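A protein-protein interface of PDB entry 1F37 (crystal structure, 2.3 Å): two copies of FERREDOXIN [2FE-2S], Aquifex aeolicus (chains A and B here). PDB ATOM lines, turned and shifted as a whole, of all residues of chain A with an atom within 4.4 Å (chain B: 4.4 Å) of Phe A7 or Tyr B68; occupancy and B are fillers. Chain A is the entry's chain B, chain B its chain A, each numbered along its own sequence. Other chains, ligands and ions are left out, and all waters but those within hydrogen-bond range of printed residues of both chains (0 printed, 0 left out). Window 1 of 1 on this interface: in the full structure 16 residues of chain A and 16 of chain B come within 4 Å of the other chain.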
ATOM      1  N   PHE A   3     -12.515  18.237  18.532  1.00  0.00           N
ATOM      2  CA  PHE A   3     -11.080  18.441  18.546  1.00  0.00           C
ATOM      3  C   PHE A   3     -10.635  19.128  19.828  1.00  0.00           C
ATOM      4  O   PHE A   3     -11.269  20.083  20.283  1.00  0.00           O
ATOM      5  CB  PHE A   3     -10.685  19.283  17.326  1.00  0.00           C
ATOM      6  CG  PHE A   3      -9.242  19.698  17.312  1.00  0.00           C
ATOM      7  CD1 PHE A   3      -8.229  18.743  17.285  1.00  0.00           C
ATOM      8  CD2 PHE A   3      -8.890  21.044  17.416  1.00  0.00           C
ATOM      9  CE1 PHE A   3      -6.884  19.121  17.375  1.00  0.00           C
ATOM     10  CE2 PHE A   3      -7.544  21.428  17.507  1.00  0.00           C
ATOM     11  CZ  PHE A   3      -6.550  20.465  17.489  1.00  0.00           C
ATOM     12  N   HIS A   5      -7.009  20.589  21.772  1.00  0.00           N
ATOM     13  CA  HIS A   5      -5.597  20.928  21.562  1.00  0.00           C
ATOM     14  C   HIS A   5      -4.909  21.100  22.953  1.00  0.00           C
ATOM     15  O   HIS A   5      -5.300  21.947  23.756  1.00  0.00           O
ATOM     16  CB  HIS A   5      -5.519  22.216  20.705  1.00  0.00           C
ATOM     17  CG  HIS A   5      -4.230  22.371  19.965  1.00  0.00           C
ATOM     18  ND1 HIS A   5      -4.082  23.247  18.909  1.00  0.00           N
ATOM     19  CD2 HIS A   5      -3.019  21.789  20.146  1.00  0.00           C
ATOM     20  CE1 HIS A   5      -2.828  23.197  18.465  1.00  0.00           C
ATOM     21  NE2 HIS A   5      -2.166  22.315  19.206  1.00  0.00           N
ATOM     22  N   VAL A   6      -3.903  20.282  23.248  1.00  0.00           N
ATOM     23  CA  VAL A   6      -3.226  20.323  24.550  1.00  0.00           C
ATOM     24  C   VAL A   6      -1.841  20.957  24.402  1.00  0.00           C
ATOM     25  O   VAL A   6      -1.059  20.512  23.566  1.00  0.00           O
ATOM     26  CB  VAL A   6      -3.070  18.897  25.100  1.00  0.00           C
ATOM     27  CG1 VAL A   6      -2.325  18.904  26.445  1.00  0.00           C
ATOM     28  CG2 VAL A   6      -4.467  18.256  25.283  1.00  0.00           C
ATOM     29  N   PHE A   7      -1.562  22.009  25.181  1.00  0.00           N
ATOM     30  CA  PHE A   7      -0.273  22.706  25.124  1.00  0.00           C
ATOM     31  C   PHE A   7       0.456  22.487  26.433  1.00  0.00           C
ATOM     32  O   PHE A   7      -0.053  22.823  27.479  1.00  0.00           O
ATOM     33  CB  PHE A   7      -0.458  24.217  24.872  1.00  0.00           C
ATOM     34  CG  PHE A   7      -0.983  24.554  23.472  1.00  0.00           C
ATOM     35  CD1 PHE A   7      -2.357  24.605  23.224  1.00  0.00           C
ATOM     36  CD2 PHE A   7      -0.115  24.862  22.437  1.00  0.00           C
ATOM     37  CE1 PHE A   7      -2.858  24.960  21.984  1.00  0.00           C
ATOM     38  CE2 PHE A   7      -0.591  25.220  21.185  1.00  0.00           C
ATOM     39  CZ  PHE A   7      -1.988  25.273  20.950  1.00  0.00           C
ATOM     40  N   VAL A   8       1.661  21.936  26.354  1.00  0.00           N
ATOM     41  CA  VAL A   8       2.476  21.626  27.533  1.00  0.00           C
ATOM     42  C   VAL A   8       3.738  22.488  27.497  1.00  0.00           C
ATOM     43  O   VAL A   8       4.494  22.402  26.528  1.00  0.00           O
ATOM     44  CB  VAL A   8       2.943  20.170  27.507  1.00  0.00           C
ATOM     45  CG1 VAL A   8       3.852  19.908  28.727  1.00  0.00           C
ATOM     46  CG2 VAL A   8       1.716  19.202  27.491  1.00  0.00           C
ATOM     47  N   CYS A   9       3.937  23.328  28.512  1.00  0.00           N
ATOM     48  CA  CYS A   9       5.128  24.195  28.558  1.00  0.00           C
ATOM     49  C   CYS A   9       6.319  23.304  28.824  1.00  0.00           C
ATOM     50  O   CYS A   9       6.259  22.471  29.743  1.00  0.00           O
ATOM     51  CB  CYS A   9       5.045  25.225  29.699  1.00  0.00           C
ATOM     52  SG  CYS A   9       6.624  26.144  29.977  1.00  0.00           S
ATOM     53  N   THR A  51       0.996  19.850  21.759  1.00  0.00           N
ATOM     54  CA  THR A  51       2.071  20.711  21.290  1.00  0.00           C
ATOM     55  C   THR A  51       2.971  21.246  22.420  1.00  0.00           C
ATOM     56  O   THR A  51       2.491  21.684  23.465  1.00  0.00           O
ATOM     57  CB  THR A  51       1.464  21.893  20.560  1.00  0.00           C
ATOM     58  OG1 THR A  51       0.653  21.417  19.469  1.00  0.00           O
ATOM     59  CG2 THR A  51       2.528  22.789  20.014  1.00  0.00           C
ATOM     60  N   THR A  53       5.457  23.899  24.100  1.00  0.00           N
ATOM     61  CA  THR A  53       5.610  25.334  23.996  1.00  0.00           C
ATOM     62  C   THR A  53       6.695  25.881  24.920  1.00  0.00           C
ATOM     63  O   THR A  53       7.259  25.154  25.786  1.00  0.00           O
ATOM     64  CB  THR A  53       4.318  26.040  24.400  1.00  0.00           C
ATOM     65  OG1 THR A  53       4.171  25.950  25.815  1.00  0.00           O
ATOM     66  CG2 THR A  53       3.100  25.328  23.800  1.00  0.00           C
ATOM     67  N   MET A  56       4.686  30.121  29.346  1.00  0.00           N
ATOM     68  CA  MET A  56       3.368  30.744  29.224  1.00  0.00           C
ATOM     69  C   MET A  56       3.046  31.646  30.455  1.00  0.00           C
ATOM     70  O   MET A  56       1.885  31.979  30.716  1.00  0.00           O
ATOM     71  CB  MET A  56       2.280  29.667  28.999  1.00  0.00           C
ATOM     72  CG  MET A  56       2.361  28.986  27.602  1.00  0.00           C
ATOM     73  SD  MET A  56       0.931  27.937  27.134  1.00  0.00           S
ATOM     74  CE  MET A  56       1.398  26.309  27.886  1.00  0.00           C
ATOM     75  N   VAL A  64       3.018  23.622  33.564  1.00  0.00           N
ATOM     76  CA  VAL A  64       1.771  24.213  33.074  1.00  0.00           C
ATOM     77  C   VAL A  64       1.200  23.528  31.786  1.00  0.00           C
ATOM     78  O   VAL A  64       1.910  23.257  30.797  1.00  0.00           O
ATOM     79  CB  VAL A  64       2.016  25.710  32.801  1.00  0.00           C
ATOM     80  CG1 VAL A  64       0.806  26.340  32.110  1.00  0.00           C
ATOM     81  CG2 VAL A  64       2.296  26.437  34.134  1.00  0.00           C
ATOM     82  N   VAL A  65      -0.091  23.259  31.791  1.00  0.00           N
ATOM     83  CA  VAL A  65      -0.731  22.625  30.645  1.00  0.00           C
ATOM     84  C   VAL A  65      -2.041  23.369  30.422  1.00  0.00           C
ATOM     85  O   VAL A  65      -2.781  23.617  31.384  1.00  0.00           O
ATOM     86  CB  VAL A  65      -1.043  21.146  30.948  1.00  0.00           C
ATOM     87  CG1 VAL A  65      -1.717  20.470  29.739  1.00  0.00           C
ATOM     88  CG2 VAL A  65       0.220  20.405  31.229  1.00  0.00           C
ATOM     89  N   VAL A  66      -2.317  23.785  29.184  1.00  0.00           N
ATOM     90  CA  VAL A  66      -3.585  24.452  28.910  1.00  0.00           C
ATOM     91  C   VAL A  66      -4.299  23.720  27.772  1.00  0.00           C
ATOM     92  O   VAL A  66      -3.707  23.441  26.728  1.00  0.00           O
ATOM     93  CB  VAL A  66      -3.429  25.966  28.557  1.00  0.00           C
ATOM     94  CG1 VAL A  66      -2.397  26.177  27.469  1.00  0.00           C
ATOM     95  CG2 VAL A  66      -4.768  26.511  28.069  1.00  0.00           C
ATOM     96  N   TYR A  68      -7.222  23.719  25.000  1.00  0.00           N
ATOM     97  CA  TYR A  68      -8.113  24.568  24.219  1.00  0.00           C
ATOM     98  C   TYR A  68      -8.976  23.631  23.370  1.00  0.00           C
ATOM     99  O   TYR A  68      -8.610  22.480  23.175  1.00  0.00           O
ATOM    100  CB  TYR A  68      -7.295  25.475  23.312  1.00  0.00           C
ATOM    101  CG  TYR A  68      -6.825  26.740  23.980  1.00  0.00           C
ATOM    102  CD1 TYR A  68      -5.472  27.006  24.133  1.00  0.00           C
ATOM    103  CD2 TYR A  68      -7.749  27.667  24.488  1.00  0.00           C
ATOM    104  CE1 TYR A  68      -5.027  28.170  24.790  1.00  0.00           C
ATOM    105  CE2 TYR A  68      -7.332  28.833  25.148  1.00  0.00           C
ATOM    106  CZ  TYR A  68      -5.964  29.076  25.302  1.00  0.00           C
ATOM    107  OH  TYR A  68      -5.545  30.178  26.010  1.00  0.00           O
ATOM    108  N   LYS B   4      -7.557  36.519  23.652  1.00  0.00           N
ATOM    109  CA  LYS B   4      -7.096  35.729  22.541  1.00  0.00           C
ATOM    110  C   LYS B   4      -5.686  35.196  22.801  1.00  0.00           C
ATOM    111  O   LYS B   4      -4.794  35.916  23.255  1.00  0.00           O
ATOM    112  CB  LYS B   4      -7.175  36.602  21.287  1.00  0.00           C
ATOM    113  CG  LYS B   4      -8.613  36.891  20.897  1.00  0.00           C
ATOM    114  CD  LYS B   4      -8.730  37.907  19.755  1.00  0.00           C
ATOM    115  CE  LYS B   4     -10.201  38.148  19.330  1.00  0.00           C
ATOM    116  NZ  LYS B   4     -10.830  36.968  18.628  1.00  0.00           N
ATOM    117  N   HIS B   5      -5.489  33.910  22.538  1.00  0.00           N
ATOM    118  CA  HIS B   5      -4.172  33.303  22.761  1.00  0.00           C
ATOM    119  C   HIS B   5      -3.622  32.929  21.388  1.00  0.00           C
ATOM    120  O   HIS B   5      -4.181  32.062  20.688  1.00  0.00           O
ATOM    121  CB  HIS B   5      -4.327  32.068  23.649  1.00  0.00           C
ATOM    122  CG  HIS B   5      -3.067  31.614  24.288  1.00  0.00           C
ATOM    123  ND1 HIS B   5      -3.050  30.798  25.407  1.00  0.00           N
ATOM    124  CD2 HIS B   5      -1.764  31.870  23.996  1.00  0.00           C
ATOM    125  CE1 HIS B   5      -1.802  30.590  25.775  1.00  0.00           C
ATOM    126  NE2 HIS B   5      -0.994  31.227  24.943  1.00  0.00           N
ATOM    127  N   PHE B   7      -0.681  31.438  19.003  1.00  0.00           N
ATOM    128  CA  PHE B   7       0.442  30.490  19.032  1.00  0.00           C
ATOM    129  C   PHE B   7       1.182  30.522  17.724  1.00  0.00           C
ATOM    130  O   PHE B   7       0.596  30.304  16.662  1.00  0.00           O
ATOM    131  CB  PHE B   7      -0.024  29.058  19.311  1.00  0.00           C
ATOM    132  CG  PHE B   7      -0.538  28.844  20.702  1.00  0.00           C
ATOM    133  CD1 PHE B   7      -1.865  29.087  21.007  1.00  0.00           C
ATOM    134  CD2 PHE B   7       0.298  28.337  21.689  1.00  0.00           C
ATOM    135  CE1 PHE B   7      -2.373  28.829  22.261  1.00  0.00           C
ATOM    136  CE2 PHE B   7      -0.187  28.066  22.957  1.00  0.00           C
ATOM    137  CZ  PHE B   7      -1.539  28.312  23.247  1.00  0.00           C
ATOM    138  N   MET B  56       3.536  22.123  15.001  1.00  0.00           N
ATOM    139  CA  MET B  56       2.120  21.850  15.144  1.00  0.00           C
ATOM    140  C   MET B  56       1.607  21.003  13.958  1.00  0.00           C
ATOM    141  O   MET B  56       0.411  20.982  13.676  1.00  0.00           O
ATOM    142  CB  MET B  56       1.327  23.157  15.285  1.00  0.00           C
ATOM    143  CG  MET B  56       1.678  23.906  16.575  1.00  0.00           C
ATOM    144  SD  MET B  56       0.570  25.257  16.989  1.00  0.00           S
ATOM    145  CE  MET B  56       1.327  26.651  16.139  1.00  0.00           C
ATOM    146  N   VAL B  66      -1.815  29.745  15.026  1.00  0.00           N
ATOM    147  CA  VAL B  66      -3.162  29.373  15.419  1.00  0.00           C
ATOM    148  C   VAL B  66      -3.629  30.362  16.481  1.00  0.00           C
ATOM    149  O   VAL B  66      -2.833  30.797  17.306  1.00  0.00           O
ATOM    150  CB  VAL B  66      -3.182  27.892  15.935  1.00  0.00           C
ATOM    151  CG1 VAL B  66      -2.074  27.673  16.881  1.00  0.00           C
ATOM    152  CG2 VAL B  66      -4.500  27.552  16.636  1.00  0.00           C
ATOM    153  N   VAL B  67      -4.904  30.764  16.428  1.00  0.00           N
ATOM    154  CA  VAL B  67      -5.456  31.687  17.415  1.00  0.00           C
ATOM    155  C   VAL B  67      -6.631  31.033  18.148  1.00  0.00           C
ATOM    156  O   VAL B  67      -7.636  30.646  17.521  1.00  0.00           O
ATOM    157  CB  VAL B  67      -5.985  32.999  16.774  1.00  0.00           C
ATOM    158  CG1 VAL B  67      -6.585  33.881  17.851  1.00  0.00           C
ATOM    159  CG2 VAL B  67      -4.872  33.751  16.055  1.00  0.00           C
ATOM    160  N   TYR B  68      -6.503  30.906  19.464  1.00  0.00           N
ATOM    161  CA  TYR B  68      -7.565  30.341  20.282  1.00  0.00           C
ATOM    162  C   TYR B  68      -8.139  31.462  21.173  1.00  0.00           C
ATOM    163  O   TYR B  68      -7.485  32.500  21.382  1.00  0.00           O
ATOM    164  CB  TYR B  68      -7.023  29.209  21.148  1.00  0.00           C
ATOM    165  CG  TYR B  68      -6.837  27.901  20.411  1.00  0.00           C
ATOM    166  CD1 TYR B  68      -5.576  27.421  20.141  1.00  0.00           C
ATOM    167  CD2 TYR B  68      -7.935  27.152  19.995  1.00  0.00           C
ATOM    168  CE1 TYR B  68      -5.397  26.206  19.459  1.00  0.00           C
ATOM    169  CE2 TYR B  68      -7.785  25.948  19.321  1.00  0.00           C
ATOM    170  CZ  TYR B  68      -6.506  25.468  19.044  1.00  0.00           C
ATOM    171  OH  TYR B  68      -6.326  24.266  18.351  1.00  0.00           O
ATOM    172  N   PRO B  69      -9.347  31.260  21.742  1.00  0.00           N
ATOM    173  CA  PRO B  69     -10.287  30.119  21.685  1.00  0.00           C
ATOM    174  C   PRO B  69     -10.887  29.904  20.301  1.00  0.00           C
ATOM    175  O   PRO B  69     -11.523  28.877  20.025  1.00  0.00           O
ATOM    176  CB  PRO B  69     -11.400  30.515  22.664  1.00  0.00           C
ATOM    177  CG  PRO B  69     -10.807  31.574  23.519  1.00  0.00           C
ATOM    178  CD  PRO B  69      -9.881  32.331  22.598  1.00  0.00           C
ATOM    179  N   ASP B  70     -10.722  30.886  19.430  1.00  0.00           N
ATOM    180  CA  ASP B  70     -11.314  30.772  18.105  1.00  0.00           C
ATOM    181  C   ASP B  70     -11.074  29.414  17.459  1.00  0.00           C
ATOM    182  O   ASP B  70     -12.011  28.733  17.082  1.00  0.00           O
ATOM    183  CB  ASP B  70     -10.782  31.871  17.183  1.00  0.00           C
ATOM    184  CG  ASP B  70     -10.921  33.270  17.782  1.00  0.00           C
ATOM    185  OD1 ASP B  70     -10.578  34.268  17.086  1.00  0.00           O
ATOM    186  OD2 ASP B  70     -11.378  33.340  18.955  1.00  0.00           O
ATOM    187  N   GLY B  71      -9.809  29.016  17.322  1.00  0.00           N
ATOM    188  CA  GLY B  71      -9.506  27.760  16.670  1.00  0.00           C
ATOM    189  C   GLY B  71      -9.244  28.062  15.196  1.00  0.00           C
ATOM    190  O   GLY B  71      -9.502  27.246  14.305  1.00  0.00           O
ATOM    191  N   TRP B  73      -6.716  28.755  12.153  1.00  0.00           N
ATOM    192  CA  TRP B  73      -5.359  28.419  11.751  1.00  0.00           C
ATOM    193  C   TRP B  73      -4.921  29.231  10.551  1.00  0.00           C
ATOM    194  O   TRP B  73      -5.610  29.255   9.541  1.00  0.00           O
ATOM    195  CB  TRP B  73      -5.263  26.923  11.425  1.00  0.00           C
ATOM    196  CG  TRP B  73      -5.538  26.000  12.610  1.00  0.00           C
ATOM    197  CD1 TRP B  73      -6.723  25.872  13.321  1.00  0.00           C
ATOM    198  CD2 TRP B  73      -4.614  25.058  13.200  1.00  0.00           C
ATOM    199  NE1 TRP B  73      -6.583  24.909  14.315  1.00  0.00           N
ATOM    200  CE2 TRP B  73      -5.303  24.400  14.260  1.00  0.00           C
ATOM    201  CE3 TRP B  73      -3.277  24.711  12.939  1.00  0.00           C
ATOM    202  CZ2 TRP B  73      -4.696  23.421  15.059  1.00  0.00           C
ATOM    203  CZ3 TRP B  73      -2.674  23.725  13.743  1.00  0.00           C
ATOM    204  CH2 TRP B  73      -3.393  23.092  14.787  1.00  0.00           C
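Among the printed residues, pairs that only touch across the chains: Phe A3 with Tyr B68 (3.2 Å), Phe A7 with Phe B7 (3.2 Å), Thr A51 with Met B56 (3.7 Å), His A5 with Trp B73 (3.7 Å), Tyr A68 with Phe B7 (3.7 Å), Tyr A68 with Tyr B68 (3.7 Å) and Phe A7 with Tyr B68 (3.8 Å).
The backbone carbonyl oxygen of Tyr B68 is in hydrogen-bond range of the backbone NH of His B5 (2.7 Å). N of His A5 is in hydrogen-bond range of O of Tyr A68, 2.8 Å away. N of Phe B7 sits at hydrogen-bond distance from O of Val B66, 2.8 Å away. The backbone NH of Thr A51 lies within hydrogen-bond range of the backbone carbonyl oxygen of Val A6 (2.8 Å). N of Val A8 lies within hydrogen-bond range of O of Thr A51 (3.0 Å). The side-chain hydroxyl (OG1) of Thr A51 sits at hydrogen-bond distance from a ring nitrogen (NE2) of His A5 (3.0 Å).
Of the printed residues of chain B, Phe A3 touches Tyr B68. Of chain B, only Phe B7 (3.2 Å) and Tyr B68 (3.8 Å) come within 4 Å of Phe A7. Cys A9 touches none of the printed residues of chain B. Val A66 touches none of the printed residues of chain B. Of the printed residues of chain B, Tyr A68 touches His B5 (2.6 Å), Phe B7 (3.7 Å) and Tyr B68 (3.7 Å). Of the printed residues of chain A, Phe B7 touches Phe A7 (3.2 Å) and Tyr A68 (3.7 Å). Printed residues of chain A within 4 Å of Met B56: Thr A51 (3.7 Å). Tyr B68 touches just these residues of chain A: Phe A3, His A5, Phe A7 and Tyr A68. Of the printed residues of chain A, Trp B73 touches His A5 (3.7 Å). The nearest printed residue of chain A that does not touch Met B56 is His A5 (4.2 Å).
OH of Tyr B68 is in hydrogen-bond range of ND1 of His A5, at 2.5 Å. OH of Tyr A68 lies within hydrogen-bond range of ND1 of His B5 (2.6 Å).
Of the 11 printed residues of chain B, 5 touch a printed residue of chain A. Hydrophobic or aromatic side chains of chain B that line the printed part of chain A: His B5, Phe B7, Met B56, Tyr B68 and Trp B73. Along chain B the printed residues that touch a printed residue of chain A span positions 5 to 73. Hydrophobic or aromatic side chains of chain A that line the printed part of chain B: Phe A3, His A5, Phe A7 and Tyr A68. Among the printed residues, 9 pairs touch across the chains.
His A5 touches Tyr B68, and with the chains exchanged Tyr A68 touches His B5. Phe B7 touches its own counterpart, Phe A7. Phe A7 touches Tyr B68, and with the chains exchanged Tyr A68 touches Phe B7. Tyr A68 touches its own counterpart, Tyr B68.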
